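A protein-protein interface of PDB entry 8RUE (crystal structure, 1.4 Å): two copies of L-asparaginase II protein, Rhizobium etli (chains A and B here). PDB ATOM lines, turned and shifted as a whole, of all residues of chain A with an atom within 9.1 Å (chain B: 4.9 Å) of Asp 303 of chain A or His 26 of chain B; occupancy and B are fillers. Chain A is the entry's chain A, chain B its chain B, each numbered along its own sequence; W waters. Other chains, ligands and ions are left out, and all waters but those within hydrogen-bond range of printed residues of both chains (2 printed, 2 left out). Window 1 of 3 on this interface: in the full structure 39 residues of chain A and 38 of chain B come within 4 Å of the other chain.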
ATOM      1  N   ASP A  12     -27.251 -12.737  15.426  1.00  0.00           N
ATOM      2  CA  ASP A  12     -25.803 -12.670  15.316  1.00  0.00           C
ATOM      3  C   ASP A  12     -25.178 -13.806  16.118  1.00  0.00           C
ATOM      4  O   ASP A  12     -25.454 -13.947  17.315  1.00  0.00           O
ATOM      5  CB  ASP A  12     -25.340 -11.314  15.850  1.00  0.00           C
ATOM      6  CG  ASP A  12     -25.793 -10.152  14.960  1.00  0.00           C
ATOM      7  OD1 ASP A  12     -25.531 -10.189  13.745  1.00  0.00           O
ATOM      8  OD2 ASP A  12     -26.409  -9.185  15.453  1.00  0.00           O
ATOM      9  N   PHE A  13     -24.311 -14.596  15.468  1.00  0.00           N
ATOM     10  CA  PHE A  13     -23.760 -15.791  16.069  1.00  0.00           C
ATOM     11  C   PHE A  13     -22.255 -15.849  15.906  1.00  0.00           C
ATOM     12  O   PHE A  13     -21.681 -15.322  14.946  1.00  0.00           O
ATOM     13  CB  PHE A  13     -24.365 -17.064  15.417  1.00  0.00           C
ATOM     14  CG  PHE A  13     -25.806 -17.244  15.751  1.00  0.00           C
ATOM     15  CD1 PHE A  13     -26.185 -17.900  16.912  1.00  0.00           C
ATOM     16  CD2 PHE A  13     -26.779 -16.691  14.949  1.00  0.00           C
ATOM     17  CE1 PHE A  13     -27.521 -18.035  17.254  1.00  0.00           C
ATOM     18  CE2 PHE A  13     -28.137 -16.839  15.275  1.00  0.00           C
ATOM     19  CZ  PHE A  13     -28.497 -17.512  16.433  1.00  0.00           C
ATOM     20  N   VAL A  14     -21.630 -16.518  16.860  1.00  0.00           N
ATOM     21  CA  VAL A  14     -20.309 -17.102  16.686  1.00  0.00           C
ATOM     22  C   VAL A  14     -20.515 -18.613  16.564  1.00  0.00           C
ATOM     23  O   VAL A  14     -21.352 -19.180  17.268  1.00  0.00           O
ATOM     24  CB  VAL A  14     -19.346 -16.693  17.828  1.00  0.00           C
ATOM     25  CG1 VAL A  14     -19.897 -17.028  19.210  1.00  0.00           C
ATOM     26  CG2 VAL A  14     -18.011 -17.325  17.610  1.00  0.00           C
ATOM     27  N   ASN A  24     -21.238 -26.123  17.258  1.00  0.00           N
ATOM     28  CA  ASN A  24     -22.085 -25.329  18.145  1.00  0.00           C
ATOM     29  C   ASN A  24     -22.249 -23.929  17.569  1.00  0.00           C
ATOM     30  O   ASN A  24     -21.414 -23.455  16.802  1.00  0.00           O
ATOM     31  CB  ASN A  24     -21.416 -25.171  19.511  1.00  0.00           C
ATOM     32  CG  ASN A  24     -21.104 -26.501  20.193  1.00  0.00           C
ATOM     33  OD1 ASN A  24     -21.855 -27.463  20.097  1.00  0.00           O
ATOM     34  ND2 ASN A  24     -19.976 -26.550  20.900  1.00  0.00           N
ATOM     35  N   SER A  25     -23.338 -23.266  17.930  1.00  0.00           N
ATOM     36  CA  SER A  25     -23.489 -21.849  17.643  1.00  0.00           C
ATOM     37  C   SER A  25     -23.937 -21.134  18.909  1.00  0.00           C
ATOM     38  O   SER A  25     -24.603 -21.711  19.788  1.00  0.00           O
ATOM     39  CB  SER A  25     -24.416 -21.516  16.452  1.00  0.00           C
ATOM     40  OG  SER A  25     -25.765 -21.892  16.685  1.00  0.00           O
ATOM     41  N   HIS A  26     -23.543 -19.878  18.997  1.00  0.00           N
ATOM     42  CA  HIS A  26     -23.710 -19.092  20.207  1.00  0.00           C
ATOM     43  C   HIS A  26     -24.223 -17.728  19.821  1.00  0.00           C
ATOM     44  O   HIS A  26     -23.571 -17.014  19.051  1.00  0.00           O
ATOM     45  CB  HIS A  26     -22.357 -18.929  20.929  1.00  0.00           C
ATOM     46  CG  HIS A  26     -21.659 -20.224  21.208  1.00  0.00           C
ATOM     47  ND1 HIS A  26     -21.708 -20.853  22.437  1.00  0.00           N
ATOM     48  CD2 HIS A  26     -20.887 -21.008  20.405  1.00  0.00           C
ATOM     49  CE1 HIS A  26     -20.990 -21.971  22.372  1.00  0.00           C
ATOM     50  NE2 HIS A  26     -20.482 -22.088  21.156  1.00  0.00           N
ATOM     51  N   ARG A  27     -25.335 -17.323  20.414  1.00  0.00           N
ATOM     52  CA  ARG A  27     -25.893 -16.011  20.126  1.00  0.00           C
ATOM     53  C   ARG A  27     -25.154 -14.906  20.875  1.00  0.00           C
ATOM     54  O   ARG A  27     -24.882 -15.025  22.072  1.00  0.00           O
ATOM     55  CB  ARG A  27     -27.370 -15.966  20.487  1.00  0.00           C
ATOM     56  CG  ARG A  27     -27.978 -14.677  20.050  1.00  0.00           C
ATOM     57  CD  ARG A  27     -29.404 -14.591  20.509  1.00  0.00           C
ATOM     58  NE  ARG A  27     -30.237 -15.548  19.793  1.00  0.00           N
ATOM     59  CZ  ARG A  27     -30.721 -15.343  18.575  1.00  0.00           C
ATOM     60  NH1 ARG A  27     -30.427 -14.249  17.887  1.00  0.00           N
ATOM     61  NH2 ARG A  27     -31.523 -16.257  18.032  1.00  0.00           N
ATOM     62  N   VAL A  28     -24.824 -13.841  20.158  1.00  0.00           N
ATOM     63  CA  VAL A  28     -24.035 -12.724  20.675  1.00  0.00           C
ATOM     64  C   VAL A  28     -24.915 -11.491  20.810  1.00  0.00           C
ATOM     65  O   VAL A  28     -25.622 -11.099  19.867  1.00  0.00           O
ATOM     66  CB  VAL A  28     -22.852 -12.411  19.729  1.00  0.00           C
ATOM     67  CG1 VAL A  28     -22.010 -11.237  20.248  1.00  0.00           C
ATOM     68  CG2 VAL A  28     -21.993 -13.643  19.545  1.00  0.00           C
ATOM     69  N   HIS A  29     -24.762 -10.792  21.933  1.00  0.00           N
ATOM     70  CA  HIS A  29     -25.347  -9.478  22.117  1.00  0.00           C
ATOM     71  C   HIS A  29     -24.208  -8.508  22.415  1.00  0.00           C
ATOM     72  O   HIS A  29     -23.289  -8.828  23.180  1.00  0.00           O
ATOM     73  CB  HIS A  29     -26.310  -9.478  23.322  1.00  0.00           C
ATOM     74  CG  HIS A  29     -27.391 -10.501  23.215  1.00  0.00           C
ATOM     75  ND1 HIS A  29     -28.471 -10.334  22.385  1.00  0.00           N
ATOM     76  CD2 HIS A  29     -27.543 -11.710  23.810  1.00  0.00           C
ATOM     77  CE1 HIS A  29     -29.264 -11.388  22.485  1.00  0.00           C
ATOM     78  NE2 HIS A  29     -28.722 -12.240  23.344  1.00  0.00           N
ATOM     79  N   ARG A  48     -30.498  -6.021  26.130  1.00  0.00           N
ATOM     80  CA  ARG A  48     -30.848  -7.217  26.875  1.00  0.00           C
ATOM     81  C   ARG A  48     -30.616  -7.010  28.370  1.00  0.00           C
ATOM     82  O   ARG A  48     -29.509  -6.636  28.802  1.00  0.00           O
ATOM     83  CB  ARG A  48     -29.942  -8.357  26.408  1.00  0.00           C
ATOM     84  CG  ARG A  48     -30.186  -9.674  27.134  1.00  0.00           C
ATOM     85  CD  ARG A  48     -29.039 -10.672  26.873  1.00  0.00           C
ATOM     86  NE  ARG A  48     -29.273 -12.033  27.378  1.00  0.00           N
ATOM     87  CZ  ARG A  48     -28.993 -12.427  28.610  1.00  0.00           C
ATOM     88  NH1 ARG A  48     -28.503 -11.587  29.510  1.00  0.00           N
ATOM     89  NH2 ARG A  48     -29.215 -13.695  28.957  1.00  0.00           N
ATOM     90  N   ALA A 272     -18.861 -13.257  35.176  1.00  0.00           N
ATOM     91  CA  ALA A 272     -19.242 -14.669  35.105  1.00  0.00           C
ATOM     92  C   ALA A 272     -20.443 -14.860  34.186  1.00  0.00           C
ATOM     93  O   ALA A 272     -21.285 -13.957  34.025  1.00  0.00           O
ATOM     94  CB  ALA A 272     -19.603 -15.183  36.505  1.00  0.00           C
ATOM     95  N   ASP A 273     -20.509 -16.055  33.587  1.00  0.00           N
ATOM     96  CA  ASP A 273     -21.533 -16.413  32.605  1.00  0.00           C
ATOM     97  C   ASP A 273     -21.426 -15.569  31.337  1.00  0.00           C
ATOM     98  O   ASP A 273     -22.413 -15.324  30.615  1.00  0.00           O
ATOM     99  CB  ASP A 273     -22.943 -16.523  33.208  1.00  0.00           C
ATOM    100  CG  ASP A 273     -23.066 -17.764  34.087  1.00  0.00           C
ATOM    101  OD1 ASP A 273     -22.869 -18.887  33.571  1.00  0.00           O
ATOM    102  OD2 ASP A 273     -23.340 -17.653  35.298  1.00  0.00           O
ATOM    103  N   ALA A 274     -20.190 -15.156  31.036  1.00  0.00           N
ATOM    104  CA  ALA A 274     -19.818 -14.678  29.705  1.00  0.00           C
ATOM    105  C   ALA A 274     -20.403 -13.307  29.371  1.00  0.00           C
ATOM    106  O   ALA A 274     -20.996 -13.105  28.306  1.00  0.00           O
ATOM    107  CB  ALA A 274     -20.092 -15.713  28.599  1.00  0.00           C
ATOM    108  N   SER A 275     -20.167 -12.332  30.254  1.00  0.00           N
ATOM    109  CA  SER A 275     -20.278 -10.928  29.888  1.00  0.00           C
ATOM    110  C   SER A 275     -18.893 -10.301  29.888  1.00  0.00           C
ATOM    111  O   SER A 275     -17.977 -10.766  30.570  1.00  0.00           O
ATOM    112  CB  SER A 275     -21.209 -10.142  30.825  1.00  0.00           C
ATOM    113  OG  SER A 275     -22.541 -10.616  30.737  1.00  0.00           O
ATOM    114  N   LYS A 300     -22.440  -9.920  25.726  1.00  0.00           N
ATOM    115  CA  LYS A 300     -22.957 -11.073  26.470  1.00  0.00           C
ATOM    116  C   LYS A 300     -23.115 -12.208  25.472  1.00  0.00           C
ATOM    117  O   LYS A 300     -23.726 -12.011  24.415  1.00  0.00           O
ATOM    118  CB  LYS A 300     -24.338 -10.772  27.110  1.00  0.00           C
ATOM    119  CG  LYS A 300     -25.169 -12.012  27.605  1.00  0.00           C
ATOM    120  CD  LYS A 300     -24.596 -12.762  28.803  1.00  0.00           C
ATOM    121  CE  LYS A 300     -25.528 -13.948  29.161  1.00  0.00           C
ATOM    122  NZ  LYS A 300     -25.063 -14.731  30.341  1.00  0.00           N
ATOM    123  N   ILE A 301     -22.572 -13.381  25.790  1.00  0.00           N
ATOM    124  CA  ILE A 301     -22.855 -14.598  25.018  1.00  0.00           C
ATOM    125  C   ILE A 301     -24.053 -15.252  25.683  1.00  0.00           C
ATOM    126  O   ILE A 301     -23.994 -15.588  26.870  1.00  0.00           O
ATOM    127  CB  ILE A 301     -21.657 -15.563  25.017  1.00  0.00           C
ATOM    128  CG1 ILE A 301     -20.399 -14.889  24.469  1.00  0.00           C
ATOM    129  CG2 ILE A 301     -21.998 -16.850  24.252  1.00  0.00           C
ATOM    130  CD1 ILE A 301     -20.534 -14.466  23.001  1.00  0.00           C
ATOM    131  N   GLU A 302     -25.150 -15.422  24.922  1.00  0.00           N
ATOM    132  CA  GLU A 302     -26.447 -15.776  25.513  1.00  0.00           C
ATOM    133  C   GLU A 302     -26.385 -17.057  26.344  1.00  0.00           C
ATOM    134  O   GLU A 302     -27.023 -17.148  27.414  1.00  0.00           O
ATOM    135  CB  GLU A 302     -27.485 -15.902  24.399  1.00  0.00           C
ATOM    136  CG  GLU A 302     -28.869 -16.299  24.901  1.00  0.00           C
ATOM    137  CD  GLU A 302     -29.483 -15.224  25.782  1.00  0.00           C
ATOM    138  OE1 GLU A 302     -29.240 -14.057  25.478  1.00  0.00           O
ATOM    139  OE2 GLU A 302     -30.233 -15.521  26.755  1.00  0.00           O
ATOM    140  N   ASP A 303     -25.609 -18.053  25.894  1.00  0.00           N
ATOM    141  CA  ASP A 303     -25.521 -19.337  26.586  1.00  0.00           C
ATOM    142  C   ASP A 303     -24.403 -19.403  27.623  1.00  0.00           C
ATOM    143  O   ASP A 303     -24.244 -20.448  28.266  1.00  0.00           O
ATOM    144  CB  ASP A 303     -25.278 -20.441  25.538  1.00  0.00           C
ATOM    145  CG  ASP A 303     -24.068 -20.117  24.662  1.00  0.00           C
ATOM    146  OD1 ASP A 303     -22.938 -20.466  25.042  1.00  0.00           O
ATOM    147  OD2 ASP A 303     -24.230 -19.421  23.653  1.00  0.00           O
ATOM    148  N   GLY A 304     -23.601 -18.353  27.809  1.00  0.00           N
ATOM    149  CA  GLY A 304     -22.624 -18.336  28.882  1.00  0.00           C
ATOM    150  C   GLY A 304     -21.239 -18.876  28.580  1.00  0.00           C
ATOM    151  O   GLY A 304     -20.450 -19.011  29.524  1.00  0.00           O
ATOM    152  N   ASN A 305     -20.891 -19.170  27.322  1.00  0.00           N
ATOM    153  CA  ASN A 305     -19.599 -19.810  27.032  1.00  0.00           C
ATOM    154  C   ASN A 305     -18.450 -18.786  27.029  1.00  0.00           C
ATOM    155  O   ASN A 305     -18.425 -17.852  26.219  1.00  0.00           O
ATOM    156  CB  ASN A 305     -19.672 -20.510  25.675  1.00  0.00           C
ATOM    157  CG  ASN A 305     -18.439 -21.334  25.375  1.00  0.00           C
ATOM    158  OD1 ASN A 305     -17.390 -20.783  25.071  1.00  0.00           O
ATOM    159  ND2 ASN A 305     -18.548 -22.662  25.457  1.00  0.00           N
ATOM    160  N   LEU A 306     -17.480 -19.003  27.909  1.00  0.00           N
ATOM    161  CA  LEU A 306     -16.402 -18.028  28.100  1.00  0.00           C
ATOM    162  C   LEU A 306     -15.424 -18.039  26.931  1.00  0.00           C
ATOM    163  O   LEU A 306     -14.941 -16.968  26.520  1.00  0.00           O
ATOM    164  CB  LEU A 306     -15.648 -18.284  29.410  1.00  0.00           C
ATOM    165  CG  LEU A 306     -16.364 -18.059  30.741  1.00  0.00           C
ATOM    166  CD1 LEU A 306     -15.447 -18.333  31.937  1.00  0.00           C
ATOM    167  CD2 LEU A 306     -16.891 -16.662  30.797  1.00  0.00           C
ATOM    168  N   GLU A 307     -15.089 -19.236  26.394  1.00  0.00           N
ATOM    169  CA  GLU A 307     -14.149 -19.296  25.274  1.00  0.00           C
ATOM    170  C   GLU A 307     -14.681 -18.492  24.095  1.00  0.00           C
ATOM    171  O   GLU A 307     -13.930 -17.749  23.432  1.00  0.00           O
ATOM    172  CB  GLU A 307     -13.963 -20.770  24.865  1.00  0.00           C
ATOM    173  CG  GLU A 307     -12.922 -20.981  23.788  1.00  0.00           C
ATOM    174  CD  GLU A 307     -12.871 -22.432  23.308  1.00  0.00           C
ATOM    175  OE1 GLU A 307     -13.948 -23.071  23.176  1.00  0.00           O
ATOM    176  OE2 GLU A 307     -11.766 -22.967  23.123  1.00  0.00           O
ATOM    177  N   MET A 308     -15.991 -18.603  23.838  1.00  0.00           N
ATOM    178  CA  MET A 308     -16.599 -17.848  22.744  1.00  0.00           C
ATOM    179  C   MET A 308     -16.641 -16.361  23.045  1.00  0.00           C
ATOM    180  O   MET A 308     -16.507 -15.547  22.128  1.00  0.00           O
ATOM    181  CB  MET A 308     -18.001 -18.373  22.483  1.00  0.00           C
ATOM    182  CG  MET A 308     -17.999 -19.808  21.945  1.00  0.00           C
ATOM    183  SD  MET A 308     -17.191 -19.983  20.346  1.00  0.00           S
ATOM    184  CE  MET A 308     -15.614 -20.633  20.857  1.00  0.00           C
ATOM    185  N   LEU A 309     -16.849 -15.990  24.309  1.00  0.00           N
ATOM    186  CA  LEU A 309     -16.788 -14.583  24.689  1.00  0.00           C
ATOM    187  C   LEU A 309     -15.453 -13.952  24.290  1.00  0.00           C
ATOM    188  O   LEU A 309     -15.423 -12.896  23.650  1.00  0.00           O
ATOM    189  CB  LEU A 309     -16.984 -14.448  26.192  1.00  0.00           C
ATOM    190  CG  LEU A 309     -16.899 -13.017  26.716  1.00  0.00           C
ATOM    191  CD1 LEU A 309     -18.094 -12.173  26.254  1.00  0.00           C
ATOM    192  CD2 LEU A 309     -16.751 -13.019  28.236  1.00  0.00           C
ATOM    193  N   ASP B  12     -37.733 -23.193  21.537  1.00  0.00           N
ATOM    194  CA  ASP B  12     -37.574 -24.157  22.614  1.00  0.00           C
ATOM    195  C   ASP B  12     -36.235 -23.937  23.315  1.00  0.00           C
ATOM    196  O   ASP B  12     -35.177 -24.112  22.702  1.00  0.00           O
ATOM    197  CB  ASP B  12     -37.716 -25.572  22.056  1.00  0.00           C
ATOM    198  CG  ASP B  12     -39.147 -25.856  21.591  1.00  0.00           C
ATOM    199  OD1 ASP B  12     -40.107 -25.541  22.328  1.00  0.00           O
ATOM    200  OD2 ASP B  12     -39.324 -26.380  20.480  1.00  0.00           O
ATOM    201  N   PHE B  13     -36.294 -23.588  24.604  1.00  0.00           N
ATOM    202  CA  PHE B  13     -35.115 -23.238  25.379  1.00  0.00           C
ATOM    203  C   PHE B  13     -35.112 -23.940  26.728  1.00  0.00           C
ATOM    204  O   PHE B  13     -36.172 -24.293  27.277  1.00  0.00           O
ATOM    205  CB  PHE B  13     -35.047 -21.723  25.648  1.00  0.00           C
ATOM    206  CG  PHE B  13     -34.699 -20.928  24.431  1.00  0.00           C
ATOM    207  CD1 PHE B  13     -35.675 -20.527  23.544  1.00  0.00           C
ATOM    208  CD2 PHE B  13     -33.381 -20.659  24.132  1.00  0.00           C
ATOM    209  CE1 PHE B  13     -35.335 -19.807  22.382  1.00  0.00           C
ATOM    210  CE2 PHE B  13     -33.034 -19.969  22.987  1.00  0.00           C
ATOM    211  CZ  PHE B  13     -34.003 -19.538  22.115  1.00  0.00           C
ATOM    212  N   VAL B  14     -33.894 -24.118  27.265  1.00  0.00           N
ATOM    213  CA  VAL B  14     -33.670 -24.353  28.688  1.00  0.00           C
ATOM    214  C   VAL B  14     -32.957 -23.106  29.207  1.00  0.00           C
ATOM    215  O   VAL B  14     -32.101 -22.541  28.512  1.00  0.00           O
ATOM    216  CB  VAL B  14     -32.913 -25.673  28.951  1.00  0.00           C
ATOM    217  CG1 VAL B  14     -31.575 -25.759  28.172  1.00  0.00           C
ATOM    218  CG2 VAL B  14     -32.677 -25.867  30.428  1.00  0.00           C
ATOM    219  N   ASN B  24     -28.548 -17.451  31.614  1.00  0.00           N
ATOM    220  CA  ASN B  24     -28.220 -17.972  30.299  1.00  0.00           C
ATOM    221  C   ASN B  24     -29.442 -18.657  29.721  1.00  0.00           C
ATOM    222  O   ASN B  24     -30.294 -19.150  30.457  1.00  0.00           O
ATOM    223  CB  ASN B  24     -27.109 -19.044  30.371  1.00  0.00           C
ATOM    224  CG  ASN B  24     -25.821 -18.525  31.000  1.00  0.00           C
ATOM    225  OD1 ASN B  24     -25.446 -17.376  30.827  1.00  0.00           O
ATOM    226  ND2 ASN B  24     -25.164 -19.385  31.762  1.00  0.00           N
ATOM    227  N   SER B  25     -29.507 -18.698  28.394  1.00  0.00           N
ATOM    228  CA  SER B  25     -30.525 -19.504  27.731  1.00  0.00           C
ATOM    229  C   SER B  25     -29.847 -20.331  26.647  1.00  0.00           C
ATOM    230  O   SER B  25     -28.823 -19.926  26.064  1.00  0.00           O
ATOM    231  CB  SER B  25     -31.724 -18.707  27.176  1.00  0.00           C
ATOM    232  OG  SER B  25     -31.350 -17.905  26.070  1.00  0.00           O
ATOM    233  N   HIS B  26     -30.404 -21.525  26.426  1.00  0.00           N
ATOM    234  CA  HIS B  26     -29.809 -22.541  25.557  1.00  0.00           C
ATOM    235  C   HIS B  26     -30.886 -23.103  24.649  1.00  0.00           C
ATOM    236  O   HIS B  26     -31.921 -23.587  25.132  1.00  0.00           O
ATOM    237  CB  HIS B  26     -29.203 -23.684  26.388  1.00  0.00           C
ATOM    238  CG  HIS B  26     -28.289 -23.235  27.476  1.00  0.00           C
ATOM    239  ND1 HIS B  26     -26.920 -23.256  27.337  1.00  0.00           N
ATOM    240  CD2 HIS B  26     -28.546 -22.725  28.709  1.00  0.00           C
ATOM    241  CE1 HIS B  26     -26.372 -22.790  28.454  1.00  0.00           C
ATOM    242  NE2 HIS B  26     -27.334 -22.448  29.294  1.00  0.00           N
ATOM    243  N   ARG B  27     -30.659 -23.042  23.340  1.00  0.00           N
ATOM    244  CA  ARG B  27     -31.629 -23.611  22.399  1.00  0.00           C
ATOM    245  C   ARG B  27     -31.574 -25.140  22.357  1.00  0.00           C
ATOM    246  O   ARG B  27     -30.494 -25.736  22.287  1.00  0.00           O
ATOM    247  CB  ARG B  27     -31.343 -23.080  20.997  1.00  0.00           C
ATOM    248  CG  ARG B  27     -32.407 -23.449  20.003  1.00  0.00           C
ATOM    249  CD  ARG B  27     -32.194 -22.751  18.670  1.00  0.00           C
ATOM    250  NE  ARG B  27     -32.508 -21.328  18.721  1.00  0.00           N
ATOM    251  CZ  ARG B  27     -33.735 -20.834  18.604  1.00  0.00           C
ATOM    252  NH1 ARG B  27     -34.795 -21.625  18.504  1.00  0.00           N
ATOM    253  NH2 ARG B  27     -33.904 -19.512  18.589  1.00  0.00           N
ATOM    254  N   VAL B  28     -32.745 -25.775  22.371  1.00  0.00           N
ATOM    255  CA  VAL B  28     -32.872 -27.227  22.423  1.00  0.00           C
ATOM    256  C   VAL B  28     -33.426 -27.733  21.096  1.00  0.00           C
ATOM    257  O   VAL B  28     -34.425 -27.195  20.586  1.00  0.00           O
ATOM    258  CB  VAL B  28     -33.845 -27.627  23.546  1.00  0.00           C
ATOM    259  CG1 VAL B  28     -34.023 -29.166  23.585  1.00  0.00           C
ATOM    260  CG2 VAL B  28     -33.347 -27.135  24.899  1.00  0.00           C
ATOM    261  N   ILE B 301     -28.090 -29.760  22.344  1.00  0.00           N
ATOM    262  CA  ILE B 301     -28.108 -28.393  22.873  1.00  0.00           C
ATOM    263  C   ILE B 301     -27.258 -27.535  21.933  1.00  0.00           C
ATOM    264  O   ILE B 301     -26.079 -27.832  21.730  1.00  0.00           O
ATOM    265  CB  ILE B 301     -27.570 -28.334  24.314  1.00  0.00           C
ATOM    266  CG1 ILE B 301     -28.341 -29.280  25.265  1.00  0.00           C
ATOM    267  CG2 ILE B 301     -27.649 -26.882  24.851  1.00  0.00           C
ATOM    268  CD1 ILE B 301     -29.831 -29.011  25.342  1.00  0.00           C
ATOM    269  N   ASP B 303     -25.656 -24.773  21.753  1.00  0.00           N
ATOM    270  CA  ASP B 303     -24.390 -24.170  22.164  1.00  0.00           C
ATOM    271  C   ASP B 303     -23.433 -25.157  22.836  1.00  0.00           C
ATOM    272  O   ASP B 303     -22.319 -24.767  23.168  1.00  0.00           O
ATOM    273  CB  ASP B 303     -24.681 -23.053  23.155  1.00  0.00           C
ATOM    274  CG  ASP B 303     -25.567 -23.532  24.284  1.00  0.00           C
ATOM    275  OD1 ASP B 303     -26.812 -23.491  24.130  1.00  0.00           O
ATOM    276  OD2 ASP B 303     -25.011 -24.011  25.300  1.00  0.00           O
ATOM    277  N   ASN B 305     -23.651 -27.035  25.797  1.00  0.00           N
ATOM    278  CA  ASN B 305     -23.515 -27.143  27.253  1.00  0.00           C
ATOM    279  C   ASN B 305     -24.017 -28.502  27.779  1.00  0.00           C
ATOM    280  O   ASN B 305     -25.207 -28.849  27.639  1.00  0.00           O
ATOM    281  CB  ASN B 305     -24.251 -25.975  27.915  1.00  0.00           C
ATOM    282  CG  ASN B 305     -24.056 -25.927  29.402  1.00  0.00           C
ATOM    283  OD1 ASN B 305     -24.526 -26.779  30.117  1.00  0.00           O
ATOM    284  ND2 ASN B 305     -23.335 -24.934  29.871  1.00  0.00           N
ATOM    285  N   MET B 308     -26.688 -28.570  30.811  1.00  0.00           N
ATOM    286  CA  MET B 308     -28.038 -28.339  30.303  1.00  0.00           C
ATOM    287  C   MET B 308     -28.564 -29.531  29.534  1.00  0.00           C
ATOM    288  O   MET B 308     -29.753 -29.843  29.628  1.00  0.00           O
ATOM    289  CB  MET B 308     -28.059 -27.106  29.425  1.00  0.00           C
ATOM    290  CG  MET B 308     -27.766 -25.810  30.193  1.00  0.00           C
ATOM    291  SD  MET B 308     -28.975 -25.418  31.460  1.00  0.00           S
ATOM    292  CE  MET B 308     -28.154 -26.050  32.925  1.00  0.00           C
HETATM  293  O   HOH W   1     -31.085 -18.594  19.315  1.00  0.00           O
HETATM  294  O   HOH W   2     -20.650 -24.493  25.391  1.00  0.00           O
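ND2 of Asn 24 of chain B lies within hydrogen-bond range of OD1 of Asp 273 of chain A (3.0 Å). OE2 of Glu 302 of chain A sits at hydrogen-bond distance from OG of Ser 25 of chain B, 2.7 Å away. The side-chain amide oxygen (OD1) of Asn 24 of chain B sits at hydrogen-bond distance from the side-chain amino group (NZ) of Lys 300 of chain A, at 2.7 Å.
The backbone NH (N) of Lys 300 of chain A is in hydrogen-bond range of the backbone carbonyl oxygen (O) of His 29 of chain A, at 2.9 Å. The side-chain carboxylate (OD2) of Asp 303 of chain B is in hydrogen-bond range of the backbone NH (N) of Asn 305 of chain B. OD1 of Asp 303 of chain A lies within hydrogen-bond range of ND1 of His 26 of chain A, 2.9 Å away. NE of Arg 48 of chain A is in salt-bridge range of OE1 of Glu 302 of chain A. The backbone carbonyl oxygen (O) of Asp 273 of chain A lies within hydrogen-bond range of the side-chain amino group (NZ) of Lys 300 of chain A, 2.7 Å away. The backbone carbonyl oxygen of Val 14 of chain A is in hydrogen-bond range of the backbone NH of His 26 of chain A.
O of Asp 303 of chain B touches CG of Asn 24 of chain A (3.7 Å). CA of Asp 303 of chain B touches O of Ser 25 of chain A, at 3.4 Å. His 26 of chain A touches Asp 303 of chain B (CE1 to O, 3.2 Å). Glu 302 of chain A touches Asn 24 of chain B. Asn 24 of chain B touches Asp 303 of chain A (CG to O, 3.7 Å). Ser 25 of chain B touches Asp 303 of chain A (O to CA, 3.4 Å). His 26 of chain B touches Asp 303 of chain A. Asp 303 of chain B touches Asp 303 of chain A. Gly 304 of chain A touches Asn 24 of chain B.
Printed residues of chain B within 4 Å of Asp 303 of chain A: Asn 24, Ser 25, His 26 and Asp 303. Printed residues of chain B within 4 Å of Glu 302 of chain A: Asn 24 (3.2 Å) and Ser 25 (2.7 Å). Printed residues of chain B within 4 Å of Asp 273 of chain A: Asn 24 (3.0 Å). Printed residues of chain A within 4 Å of Ser 25 of chain B: Glu 302 and Asp 303. Printed residues of chain B within 4 Å of Asn 24 of chain A: Asp 303. Printed residues of chain B within 4 Å of Ser 25 of chain A: Asp 303 (3.4 Å). Arg 48 of chain A touches none of the printed residues of chain B. The nearest printed residue of chain B that does not touch Asp 273 of chain A is Asn 305 of chain B (7.1 Å).
Of the 24 printed residues of chain A, 8 touch a printed residue of chain B. Printed residues of chain A that touch a printed residue of chain B: Asn 24, Ser 25, His 26, Asp 273, Lys 300, Glu 302, Asp 303 and Gly 304. Hydrophobic or aromatic side chains of chain A within 4 Å of the printed part of chain B: His 26. Hydrophobic or aromatic side chains of chain B within 4 Å of the printed part of chain A: His 26. Among the printed residues, 12 pairs touch across the chains.
Asn 24 of chain A touches Asp 303 of chain B, and with the chains exchanged Asp 303 of chain A touches Asn 24 of chain B. Ser 25 of chain A touches Asp 303 of chain B, and with the chains exchanged Asp 303 of chain A touches Ser 25 of chain B. His 26 of chain A touches Asp 303 of chain B, and with the chains exchanged Asp 303 of chain A touches His 26 of chain B. Asp 303 of chain A touches its own counterpart, Asp 303 of chain B. Of the 12 pairs that touch across the chains among the printed residues, 7 have their exchanged pair printed and touching as well.
Water W1 lies within hydrogen-bond range of NH2 of Arg 27 of chain A (2.7 Å) and NH2 of Arg 27 of chain B (3.1 Å). Water W2 lies within hydrogen-bond range of ND2 of Asn 305 of chain A (2.8 Å) and O of Asp 303 of chain B (2.8 Å).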
